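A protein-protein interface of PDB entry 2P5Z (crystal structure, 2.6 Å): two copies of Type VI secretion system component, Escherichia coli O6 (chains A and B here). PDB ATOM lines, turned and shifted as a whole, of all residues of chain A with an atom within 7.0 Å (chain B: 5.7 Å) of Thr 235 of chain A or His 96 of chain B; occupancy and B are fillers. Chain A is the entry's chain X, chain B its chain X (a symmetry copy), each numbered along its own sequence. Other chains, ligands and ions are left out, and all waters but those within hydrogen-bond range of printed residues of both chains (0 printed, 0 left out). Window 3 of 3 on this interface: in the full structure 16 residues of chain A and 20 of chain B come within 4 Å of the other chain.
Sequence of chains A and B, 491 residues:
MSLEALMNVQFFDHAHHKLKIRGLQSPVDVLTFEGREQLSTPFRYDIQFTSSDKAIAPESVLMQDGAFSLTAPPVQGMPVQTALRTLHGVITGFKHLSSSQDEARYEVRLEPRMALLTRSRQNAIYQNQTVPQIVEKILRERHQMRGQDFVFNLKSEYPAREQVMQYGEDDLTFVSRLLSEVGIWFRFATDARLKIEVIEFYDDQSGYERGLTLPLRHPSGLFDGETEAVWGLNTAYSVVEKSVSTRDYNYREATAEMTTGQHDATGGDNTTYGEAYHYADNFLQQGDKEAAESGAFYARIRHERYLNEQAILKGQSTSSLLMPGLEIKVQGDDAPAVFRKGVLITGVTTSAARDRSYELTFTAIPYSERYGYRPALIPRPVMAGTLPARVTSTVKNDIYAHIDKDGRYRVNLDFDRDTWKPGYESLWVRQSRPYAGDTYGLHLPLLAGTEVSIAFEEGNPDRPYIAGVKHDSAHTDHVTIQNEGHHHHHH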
ATOM      1  N   GLY A 232       0.387  35.226  -7.191  1.00  0.00           N
ATOM      2  CA  GLY A 232       1.094  33.940  -7.260  1.00  0.00           C
ATOM      3  C   GLY A 232       1.290  33.261  -5.906  1.00  0.00           C
ATOM      4  O   GLY A 232       2.251  32.508  -5.718  1.00  0.00           O
ATOM      5  N   LEU A 233       0.384  33.535  -4.968  1.00  0.00           N
ATOM      6  CA  LEU A 233       0.533  33.074  -3.601  1.00  0.00           C
ATOM      7  C   LEU A 233       0.473  31.561  -3.492  1.00  0.00           C
ATOM      8  O   LEU A 233      -0.363  30.918  -4.132  1.00  0.00           O
ATOM      9  CB  LEU A 233      -0.510  33.700  -2.682  1.00  0.00           C
ATOM     10  CG  LEU A 233      -0.560  35.228  -2.606  1.00  0.00           C
ATOM     11  CD1 LEU A 233      -1.487  35.686  -1.488  1.00  0.00           C
ATOM     12  CD2 LEU A 233       0.822  35.842  -2.412  1.00  0.00           C
ATOM     13  N   ASN A 234       1.383  31.012  -2.687  1.00  0.00           N
ATOM     14  CA  ASN A 234       1.468  29.577  -2.461  1.00  0.00           C
ATOM     15  C   ASN A 234       2.073  29.208  -1.094  1.00  0.00           C
ATOM     16  O   ASN A 234       2.744  30.024  -0.451  1.00  0.00           O
ATOM     17  CB  ASN A 234       2.233  28.910  -3.591  1.00  0.00           C
ATOM     18  CG  ASN A 234       3.682  29.318  -3.631  1.00  0.00           C
ATOM     19  OD1 ASN A 234       4.541  28.600  -3.133  1.00  0.00           O
ATOM     20  ND2 ASN A 234       3.967  30.472  -4.231  1.00  0.00           N
ATOM     21  N   THR A 235       1.802  27.983  -0.646  1.00  0.00           N
ATOM     22  CA  THR A 235       2.206  27.541   0.672  1.00  0.00           C
ATOM     23  C   THR A 235       2.921  26.230   0.570  1.00  0.00           C
ATOM     24  O   THR A 235       2.803  25.530  -0.429  1.00  0.00           O
ATOM     25  CB  THR A 235       1.029  27.231   1.579  1.00  0.00           C
ATOM     26  OG1 THR A 235       0.332  26.115   1.034  1.00  0.00           O
ATOM     27  CG2 THR A 235       0.090  28.420   1.778  1.00  0.00           C
ATOM     28  N   ALA A 236       3.657  25.899   1.627  1.00  0.00           N
ATOM     29  CA  ALA A 236       4.359  24.628   1.731  1.00  0.00           C
ATOM     30  C   ALA A 236       4.427  24.267   3.202  1.00  0.00           C
ATOM     31  O   ALA A 236       4.736  25.115   4.048  1.00  0.00           O
ATOM     32  CB  ALA A 236       5.761  24.718   1.138  1.00  0.00           C
ATOM     33  N   TYR A 237       4.105  23.021   3.508  1.00  0.00           N
ATOM     34  CA  TYR A 237       4.080  22.555   4.882  1.00  0.00           C
ATOM     35  C   TYR A 237       4.698  21.203   4.863  1.00  0.00           C
ATOM     36  O   TYR A 237       4.433  20.400   3.969  1.00  0.00           O
ATOM     37  CB  TYR A 237       2.664  22.439   5.417  1.00  0.00           C
ATOM     38  CG  TYR A 237       1.953  23.748   5.630  1.00  0.00           C
ATOM     39  CD1 TYR A 237       1.265  24.378   4.585  1.00  0.00           C
ATOM     40  CD2 TYR A 237       1.911  24.336   6.881  1.00  0.00           C
ATOM     41  CE1 TYR A 237       0.589  25.576   4.791  1.00  0.00           C
ATOM     42  CE2 TYR A 237       1.225  25.529   7.089  1.00  0.00           C
ATOM     43  CZ  TYR A 237       0.581  26.141   6.040  1.00  0.00           C
ATOM     44  OH  TYR A 237      -0.082  27.324   6.254  1.00  0.00           O
ATOM     45  N   ALA A 311       6.318  25.674   7.971  1.00  0.00           N
ATOM     46  CA  ALA A 311       5.343  26.384   7.164  1.00  0.00           C
ATOM     47  C   ALA A 311       5.997  27.471   6.331  1.00  0.00           C
ATOM     48  O   ALA A 311       6.222  28.570   6.826  1.00  0.00           O
ATOM     49  CB  ALA A 311       4.278  26.984   8.046  1.00  0.00           C
ATOM     50  N   ILE A 312       6.287  27.184   5.065  1.00  0.00           N
ATOM     51  CA  ILE A 312       6.815  28.223   4.179  1.00  0.00           C
ATOM     52  C   ILE A 312       5.730  28.862   3.281  1.00  0.00           C
ATOM     53  O   ILE A 312       5.009  28.183   2.537  1.00  0.00           O
ATOM     54  CB  ILE A 312       8.038  27.735   3.356  1.00  0.00           C
ATOM     55  CG1 ILE A 312       9.111  27.165   4.297  1.00  0.00           C
ATOM     56  CG2 ILE A 312       8.640  28.878   2.559  1.00  0.00           C
ATOM     57  CD1 ILE A 312      10.238  26.376   3.578  1.00  0.00           C
ATOM     58  N   LEU A 313       5.625  30.179   3.372  1.00  0.00           N
ATOM     59  CA  LEU A 313       4.705  30.926   2.555  1.00  0.00           C
ATOM     60  C   LEU A 313       5.476  31.628   1.442  1.00  0.00           C
ATOM     61  O   LEU A 313       6.512  32.247   1.696  1.00  0.00           O
ATOM     62  CB  LEU A 313       3.980  31.937   3.424  1.00  0.00           C
ATOM     63  CG  LEU A 313       3.308  31.285   4.633  1.00  0.00           C
ATOM     64  CD1 LEU A 313       2.458  32.275   5.361  1.00  0.00           C
ATOM     65  CD2 LEU A 313       2.446  30.097   4.234  1.00  0.00           C
ATOM     66  N   LYS A 314       4.993  31.510   0.207  1.00  0.00           N
ATOM     67  CA  LYS A 314       5.630  32.176  -0.918  1.00  0.00           C
ATOM     68  C   LYS A 314       4.682  33.038  -1.751  1.00  0.00           C
ATOM     69  O   LYS A 314       3.459  32.990  -1.593  1.00  0.00           O
ATOM     70  CB  LYS A 314       6.347  31.183  -1.814  1.00  0.00           C
ATOM     71  CG  LYS A 314       7.578  30.546  -1.209  1.00  0.00           C
ATOM     72  CD  LYS A 314       8.509  30.061  -2.308  1.00  0.00           C
ATOM     73  CE  LYS A 314       9.307  28.841  -1.857  1.00  0.00           C
ATOM     74  NZ  LYS A 314       8.396  27.685  -1.525  1.00  0.00           N
ATOM     75  N   ASP A 334      -9.425  35.873  -2.475  1.00  0.00           N
ATOM     76  CA  ASP A 334      -9.238  34.559  -3.085  1.00  0.00           C
ATOM     77  C   ASP A 334      -7.881  33.994  -2.635  1.00  0.00           C
ATOM     78  O   ASP A 334      -7.475  32.899  -3.031  1.00  0.00           O
ATOM     79  CB  ASP A 334      -9.301  34.680  -4.615  1.00  0.00           C
ATOM     80  CG  ASP A 334      -9.761  33.390  -5.299  1.00  0.00           C
ATOM     81  OD1 ASP A 334     -10.062  32.401  -4.593  1.00  0.00           O
ATOM     82  OD2 ASP A 334      -9.829  33.367  -6.550  1.00  0.00           O
ATOM     83  N   ALA A 335      -7.193  34.776  -1.804  1.00  0.00           N
ATOM     84  CA  ALA A 335      -5.924  34.417  -1.190  1.00  0.00           C
ATOM     85  C   ALA A 335      -6.178  33.533   0.021  1.00  0.00           C
ATOM     86  O   ALA A 335      -7.119  33.793   0.774  1.00  0.00           O
ATOM     87  CB  ALA A 335      -5.206  35.684  -0.755  1.00  0.00           C
ATOM     88  N   PRO A 336      -5.337  32.489   0.213  1.00  0.00           N
ATOM     89  CA  PRO A 336      -5.369  31.600   1.382  1.00  0.00           C
ATOM     90  C   PRO A 336      -5.375  32.319   2.737  1.00  0.00           C
ATOM     91  O   PRO A 336      -4.920  33.463   2.841  1.00  0.00           O
ATOM     92  CB  PRO A 336      -4.101  30.761   1.213  1.00  0.00           C
ATOM     93  CG  PRO A 336      -3.891  30.715  -0.261  1.00  0.00           C
ATOM     94  CD  PRO A 336      -4.303  32.067  -0.756  1.00  0.00           C
ATOM     95  N   VAL A 338      -3.876  32.238   5.694  1.00  0.00           N
ATOM     96  CA  VAL A 338      -2.655  32.726   6.349  1.00  0.00           C
ATOM     97  C   VAL A 338      -2.236  34.110   5.885  1.00  0.00           C
ATOM     98  O   VAL A 338      -1.820  34.937   6.698  1.00  0.00           O
ATOM     99  CB  VAL A 338      -1.452  31.770   6.149  1.00  0.00           C
ATOM    100  CG1 VAL A 338      -1.351  30.781   7.296  1.00  0.00           C
ATOM    101  CG2 VAL A 338      -1.524  31.047   4.799  1.00  0.00           C
ATOM    102  N   PHE A 339      -2.372  34.361   4.585  1.00  0.00           N
ATOM    103  CA  PHE A 339      -2.006  35.645   3.990  1.00  0.00           C
ATOM    104  C   PHE A 339      -2.955  36.772   4.392  1.00  0.00           C
ATOM    105  O   PHE A 339      -2.601  37.950   4.305  1.00  0.00           O
ATOM    106  CB  PHE A 339      -1.994  35.548   2.469  1.00  0.00           C
ATOM    107  CG  PHE A 339      -0.934  34.648   1.912  1.00  0.00           C
ATOM    108  CD1 PHE A 339       0.358  35.116   1.715  1.00  0.00           C
ATOM    109  CD2 PHE A 339      -1.243  33.345   1.528  1.00  0.00           C
ATOM    110  CE1 PHE A 339       1.329  34.289   1.175  1.00  0.00           C
ATOM    111  CE2 PHE A 339      -0.273  32.510   0.978  1.00  0.00           C
ATOM    112  CZ  PHE A 339       1.013  32.979   0.803  1.00  0.00           C
ATOM    113  N   LYS B  54     -11.087  25.181  -2.536  1.00  0.00           N
ATOM    114  CA  LYS B  54     -10.035  26.180  -2.664  1.00  0.00           C
ATOM    115  C   LYS B  54      -9.351  26.514  -1.334  1.00  0.00           C
ATOM    116  O   LYS B  54      -8.651  27.520  -1.245  1.00  0.00           O
ATOM    117  CB  LYS B  54     -10.589  27.458  -3.303  1.00  0.00           C
ATOM    118  CG  LYS B  54     -11.405  27.191  -4.544  1.00  0.00           C
ATOM    119  CD  LYS B  54     -11.300  28.325  -5.547  1.00  0.00           C
ATOM    120  CE  LYS B  54     -12.016  29.580  -5.069  1.00  0.00           C
ATOM    121  NZ  LYS B  54     -11.639  30.733  -5.936  1.00  0.00           N
ATOM    122  N   ALA B  55      -9.546  25.669  -0.318  1.00  0.00           N
ATOM    123  CA  ALA B  55      -8.956  25.879   1.008  1.00  0.00           C
ATOM    124  C   ALA B  55      -8.738  24.576   1.771  1.00  0.00           C
ATOM    125  O   ALA B  55      -9.097  24.485   2.937  1.00  0.00           O
ATOM    126  CB  ALA B  55      -9.823  26.827   1.837  1.00  0.00           C
ATOM    127  N   ILE B  56      -8.171  23.562   1.117  1.00  0.00           N
ATOM    128  CA  ILE B  56      -7.749  22.356   1.825  1.00  0.00           C
ATOM    129  C   ILE B  56      -6.674  22.761   2.829  1.00  0.00           C
ATOM    130  O   ILE B  56      -5.682  23.409   2.461  1.00  0.00           O
ATOM    131  CB  ILE B  56      -7.176  21.298   0.878  1.00  0.00           C
ATOM    132  CG1 ILE B  56      -8.165  20.985  -0.249  1.00  0.00           C
ATOM    133  CG2 ILE B  56      -6.821  20.032   1.644  1.00  0.00           C
ATOM    134  CD1 ILE B  56      -7.754  19.794  -1.100  1.00  0.00           C
ATOM    135  N   PHE B  94       2.735  19.093   2.079  1.00  0.00           N
ATOM    136  CA  PHE B  94       1.538  19.573   1.469  1.00  0.00           C
ATOM    137  C   PHE B  94       1.808  20.961   0.967  1.00  0.00           C
ATOM    138  O   PHE B  94       2.385  21.790   1.684  1.00  0.00           O
ATOM    139  CB  PHE B  94       0.386  19.574   2.479  1.00  0.00           C
ATOM    140  CG  PHE B  94      -0.814  20.352   2.033  1.00  0.00           C
ATOM    141  CD1 PHE B  94      -1.657  19.851   1.048  1.00  0.00           C
ATOM    142  CD2 PHE B  94      -1.106  21.587   2.601  1.00  0.00           C
ATOM    143  CE1 PHE B  94      -2.758  20.566   0.634  1.00  0.00           C
ATOM    144  CE2 PHE B  94      -2.223  22.313   2.201  1.00  0.00           C
ATOM    145  CZ  PHE B  94      -3.050  21.795   1.218  1.00  0.00           C
ATOM    146  N   LYS B  95       1.373  21.218  -0.262  1.00  0.00           N
ATOM    147  CA  LYS B  95       1.509  22.535  -0.857  1.00  0.00           C
ATOM    148  C   LYS B  95       0.203  22.987  -1.487  1.00  0.00           C
ATOM    149  O   LYS B  95      -0.431  22.225  -2.205  1.00  0.00           O
ATOM    150  CB  LYS B  95       2.588  22.490  -1.938  1.00  0.00           C
ATOM    151  CG  LYS B  95       3.993  22.515  -1.429  1.00  0.00           C
ATOM    152  CD  LYS B  95       4.911  21.984  -2.465  1.00  0.00           C
ATOM    153  CE  LYS B  95       6.324  22.461  -2.205  1.00  0.00           C
ATOM    154  NZ  LYS B  95       7.211  21.844  -3.228  1.00  0.00           N
ATOM    155  N   HIS B  96      -0.210  24.218  -1.222  1.00  0.00           N
ATOM    156  CA  HIS B  96      -1.240  24.827  -2.050  1.00  0.00           C
ATOM    157  C   HIS B  96      -0.515  25.639  -3.130  1.00  0.00           C
ATOM    158  O   HIS B  96       0.195  26.578  -2.823  1.00  0.00           O
ATOM    159  CB  HIS B  96      -2.147  25.716  -1.203  1.00  0.00           C
ATOM    160  CG  HIS B  96      -3.320  26.302  -1.944  1.00  0.00           C
ATOM    161  ND1 HIS B  96      -4.508  26.620  -1.314  1.00  0.00           N
ATOM    162  CD2 HIS B  96      -3.489  26.635  -3.249  1.00  0.00           C
ATOM    163  CE1 HIS B  96      -5.349  27.129  -2.194  1.00  0.00           C
ATOM    164  NE2 HIS B  96      -4.756  27.149  -3.374  1.00  0.00           N
ATOM    165  N   LEU B  97      -0.701  25.284  -4.391  1.00  0.00           N
ATOM    166  CA  LEU B  97       0.077  25.894  -5.474  1.00  0.00           C
ATOM    167  C   LEU B  97      -0.534  27.142  -6.121  1.00  0.00           C
ATOM    168  O   LEU B  97       0.160  28.121  -6.338  1.00  0.00           O
ATOM    169  CB  LEU B  97       0.388  24.851  -6.536  1.00  0.00           C
ATOM    170  CG  LEU B  97       1.429  23.892  -5.999  1.00  0.00           C
ATOM    171  CD1 LEU B  97       1.674  22.767  -6.955  1.00  0.00           C
ATOM    172  CD2 LEU B  97       2.698  24.678  -5.748  1.00  0.00           C
ATOM    173  N   SER B  98      -1.823  27.104  -6.441  1.00  0.00           N
ATOM    174  CA  SER B  98      -2.504  28.242  -7.079  1.00  0.00           C
ATOM    175  C   SER B  98      -3.993  28.089  -6.920  1.00  0.00           C
ATOM    176  O   SER B  98      -4.469  27.055  -6.460  1.00  0.00           O
ATOM    177  CB  SER B  98      -2.180  28.341  -8.582  1.00  0.00           C
ATOM    178  OG  SER B  98      -2.493  27.130  -9.244  1.00  0.00           O
ATOM    179  N   SER B  99      -4.725  29.113  -7.329  1.00  0.00           N
ATOM    180  CA  SER B  99      -6.176  29.070  -7.290  1.00  0.00           C
ATOM    181  C   SER B  99      -6.756  29.723  -8.512  1.00  0.00           C
ATOM    182  O   SER B  99      -6.327  30.785  -8.921  1.00  0.00           O
ATOM    183  CB  SER B  99      -6.687  29.771  -6.040  1.00  0.00           C
ATOM    184  OG  SER B  99      -6.390  28.994  -4.889  1.00  0.00           O
ATOM    185  N   ALA B 104      -8.474  24.831  -7.192  1.00  0.00           N
ATOM    186  CA  ALA B 104      -7.152  25.109  -6.672  1.00  0.00           C
ATOM    187  C   ALA B 104      -6.246  23.953  -7.004  1.00  0.00           C
ATOM    188  O   ALA B 104      -6.713  22.833  -7.181  1.00  0.00           O
ATOM    189  CB  ALA B 104      -7.193  25.354  -5.186  1.00  0.00           C
ATOM    190  N   ARG B 105      -4.954  24.242  -7.119  1.00  0.00           N
ATOM    191  CA  ARG B 105      -3.944  23.239  -7.452  1.00  0.00           C
ATOM    192  C   ARG B 105      -3.165  22.934  -6.173  1.00  0.00           C
ATOM    193  O   ARG B 105      -2.852  23.841  -5.407  1.00  0.00           O
ATOM    194  CB  ARG B 105      -3.031  23.804  -8.534  1.00  0.00           C
ATOM    195  CG  ARG B 105      -2.032  22.865  -9.153  1.00  0.00           C
ATOM    196  CD  ARG B 105      -1.440  23.566 -10.353  1.00  0.00           C
ATOM    197  NE  ARG B 105       0.026  23.561 -10.375  1.00  0.00           N
ATOM    198  CZ  ARG B 105       0.792  24.654 -10.315  1.00  0.00           C
ATOM    199  NH1 ARG B 105       0.246  25.861 -10.230  1.00  0.00           N
ATOM    200  NH2 ARG B 105       2.116  24.535 -10.346  1.00  0.00           N
ATOM    201  N   TYR B 106      -2.884  21.659  -5.931  1.00  0.00           N
ATOM    202  CA  TYR B 106      -2.224  21.247  -4.699  1.00  0.00           C
ATOM    203  C   TYR B 106      -1.129  20.258  -4.992  1.00  0.00           C
ATOM    204  O   TYR B 106      -1.154  19.606  -6.036  1.00  0.00           O
ATOM    205  CB  TYR B 106      -3.199  20.587  -3.713  1.00  0.00           C
ATOM    206  CG  TYR B 106      -4.299  21.497  -3.237  1.00  0.00           C
ATOM    207  CD1 TYR B 106      -5.555  21.484  -3.848  1.00  0.00           C
ATOM    208  CD2 TYR B 106      -4.088  22.380  -2.181  1.00  0.00           C
ATOM    209  CE1 TYR B 106      -6.570  22.324  -3.420  1.00  0.00           C
ATOM    210  CE2 TYR B 106      -5.093  23.226  -1.745  1.00  0.00           C
ATOM    211  CZ  TYR B 106      -6.337  23.198  -2.372  1.00  0.00           C
ATOM    212  OH  TYR B 106      -7.349  24.040  -1.936  1.00  0.00           O
ATOM    213  N   GLU B 107      -0.179  20.130  -4.065  1.00  0.00           N
ATOM    214  CA  GLU B 107       0.798  19.052  -4.153  1.00  0.00           C
ATOM    215  C   GLU B 107       0.952  18.292  -2.838  1.00  0.00           C
ATOM    216  O   GLU B 107       0.898  18.883  -1.761  1.00  0.00           O
ATOM    217  CB  GLU B 107       2.146  19.576  -4.644  1.00  0.00           C
ATOM    218  CG  GLU B 107       3.032  18.491  -5.227  1.00  0.00           C
ATOM    219  CD  GLU B 107       4.349  19.029  -5.753  1.00  0.00           C
ATOM    220  OE1 GLU B 107       4.356  19.598  -6.863  1.00  0.00           O
ATOM    221  OE2 GLU B 107       5.384  18.873  -5.067  1.00  0.00           O
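OG1 of Thr 235 of chain A sits at hydrogen-bond distance from N of His 96 of chain B, 3.0 Å away. N of Tyr 237 of chain A sits at hydrogen-bond distance from O of Phe 94 of chain B, at 2.8 Å. OD1 of Asp 334 of chain A lies within salt-bridge range of NZ of Lys 54 of chain B (2.7 Å).
No position is printed for both chains.
The side-chain hydroxyl (OG) of Ser 99 of chain B lies within hydrogen-bond range of a ring nitrogen (NE2) of His 96 of chain B. O of Ala 236 of chain A lies within hydrogen-bond range of N of Ile 312 of chain A, at 2.8 Å. OE2 of Glu 107 of chain B lies within salt-bridge range of NZ of Lys 95 of chain B (3.9 Å). ND2 of Asn 234 of chain A is in hydrogen-bond range of O of Gly 232 of chain A, 3.0 Å away. NE2 of His 96 of chain B lies within hydrogen-bond range of O of Ser 98 of chain B (3.1 Å). The backbone carbonyl oxygen of Asn 234 of chain A lies within hydrogen-bond range of the backbone NH of Lys 314 of chain A (2.8 Å).
Of the 15 printed residues of chain A, 6 touch a printed residue of chain B. Hydrophobic or aromatic side chains of chain A that line the printed part of chain B: Ala 236 and Tyr 237. Hydrophobic or aromatic side chains of chain B within 4 Å of the printed part of chain A: His 96. Among the printed residues, 9 pairs touch across the chains. Among the printed residues, Asp or Glu carboxylates within 4 Å of a Lys or Arg side-chain nitrogen of the other chain: Asp 334 of chain A with Lys 54 of chain B.
Printed residues of chain B within 4 Å of Leu 233 of chain A: Leu 97. Thr 235 of chain A touches just these residues of chain B: Lys 95 (3.3 Å) and His 96 (3.0 Å). Printed residues of chain B within 4 Å of Ala 236 of chain A: Phe 94 (3.5 Å) and Lys 95 (3.8 Å). Printed residues of chain B within 4 Å of Tyr 237 of chain A: Phe 94 (2.8 Å). Of the printed residues of chain A, Lys 95 of chain B touches Thr 235 and Ala 236. Of chain A, only Asn 234 (3.2 Å) and Thr 235 (3.0 Å) come within 4 Å of His 96 of chain B. Of the printed residues of chain A, Leu 97 of chain B touches Leu 233 (3.6 Å) and Asn 234 (3.5 Å). Tyr 106 of chain B touches none of the printed residues of chain A. Glu 107 of chain B touches none of the printed residues of chain A. The nearest residue of chain B that does not touch Thr 235 of chain A is Phe 94 of chain B (4.3 Å). The nearest printed residue of chain B that does not touch Ala 236 of chain A is His 96 of chain B (5.1 Å).
Leu 233 of chain A touches Leu 97 of chain B. Asn 234 of chain A touches His 96 of chain B (CB to O, 3.2 Å). Leu 97 of chain B touches Asn 234 of chain A (O to CB, 3.5 Å). CA of Lys 95 of chain B touches O of Thr 235 of chain A (3.3 Å). Ala 236 of chain A touches Phe 94 of chain B (CA to O, 3.5 Å). Ala 236 of chain A touches Lys 95 of chain B.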
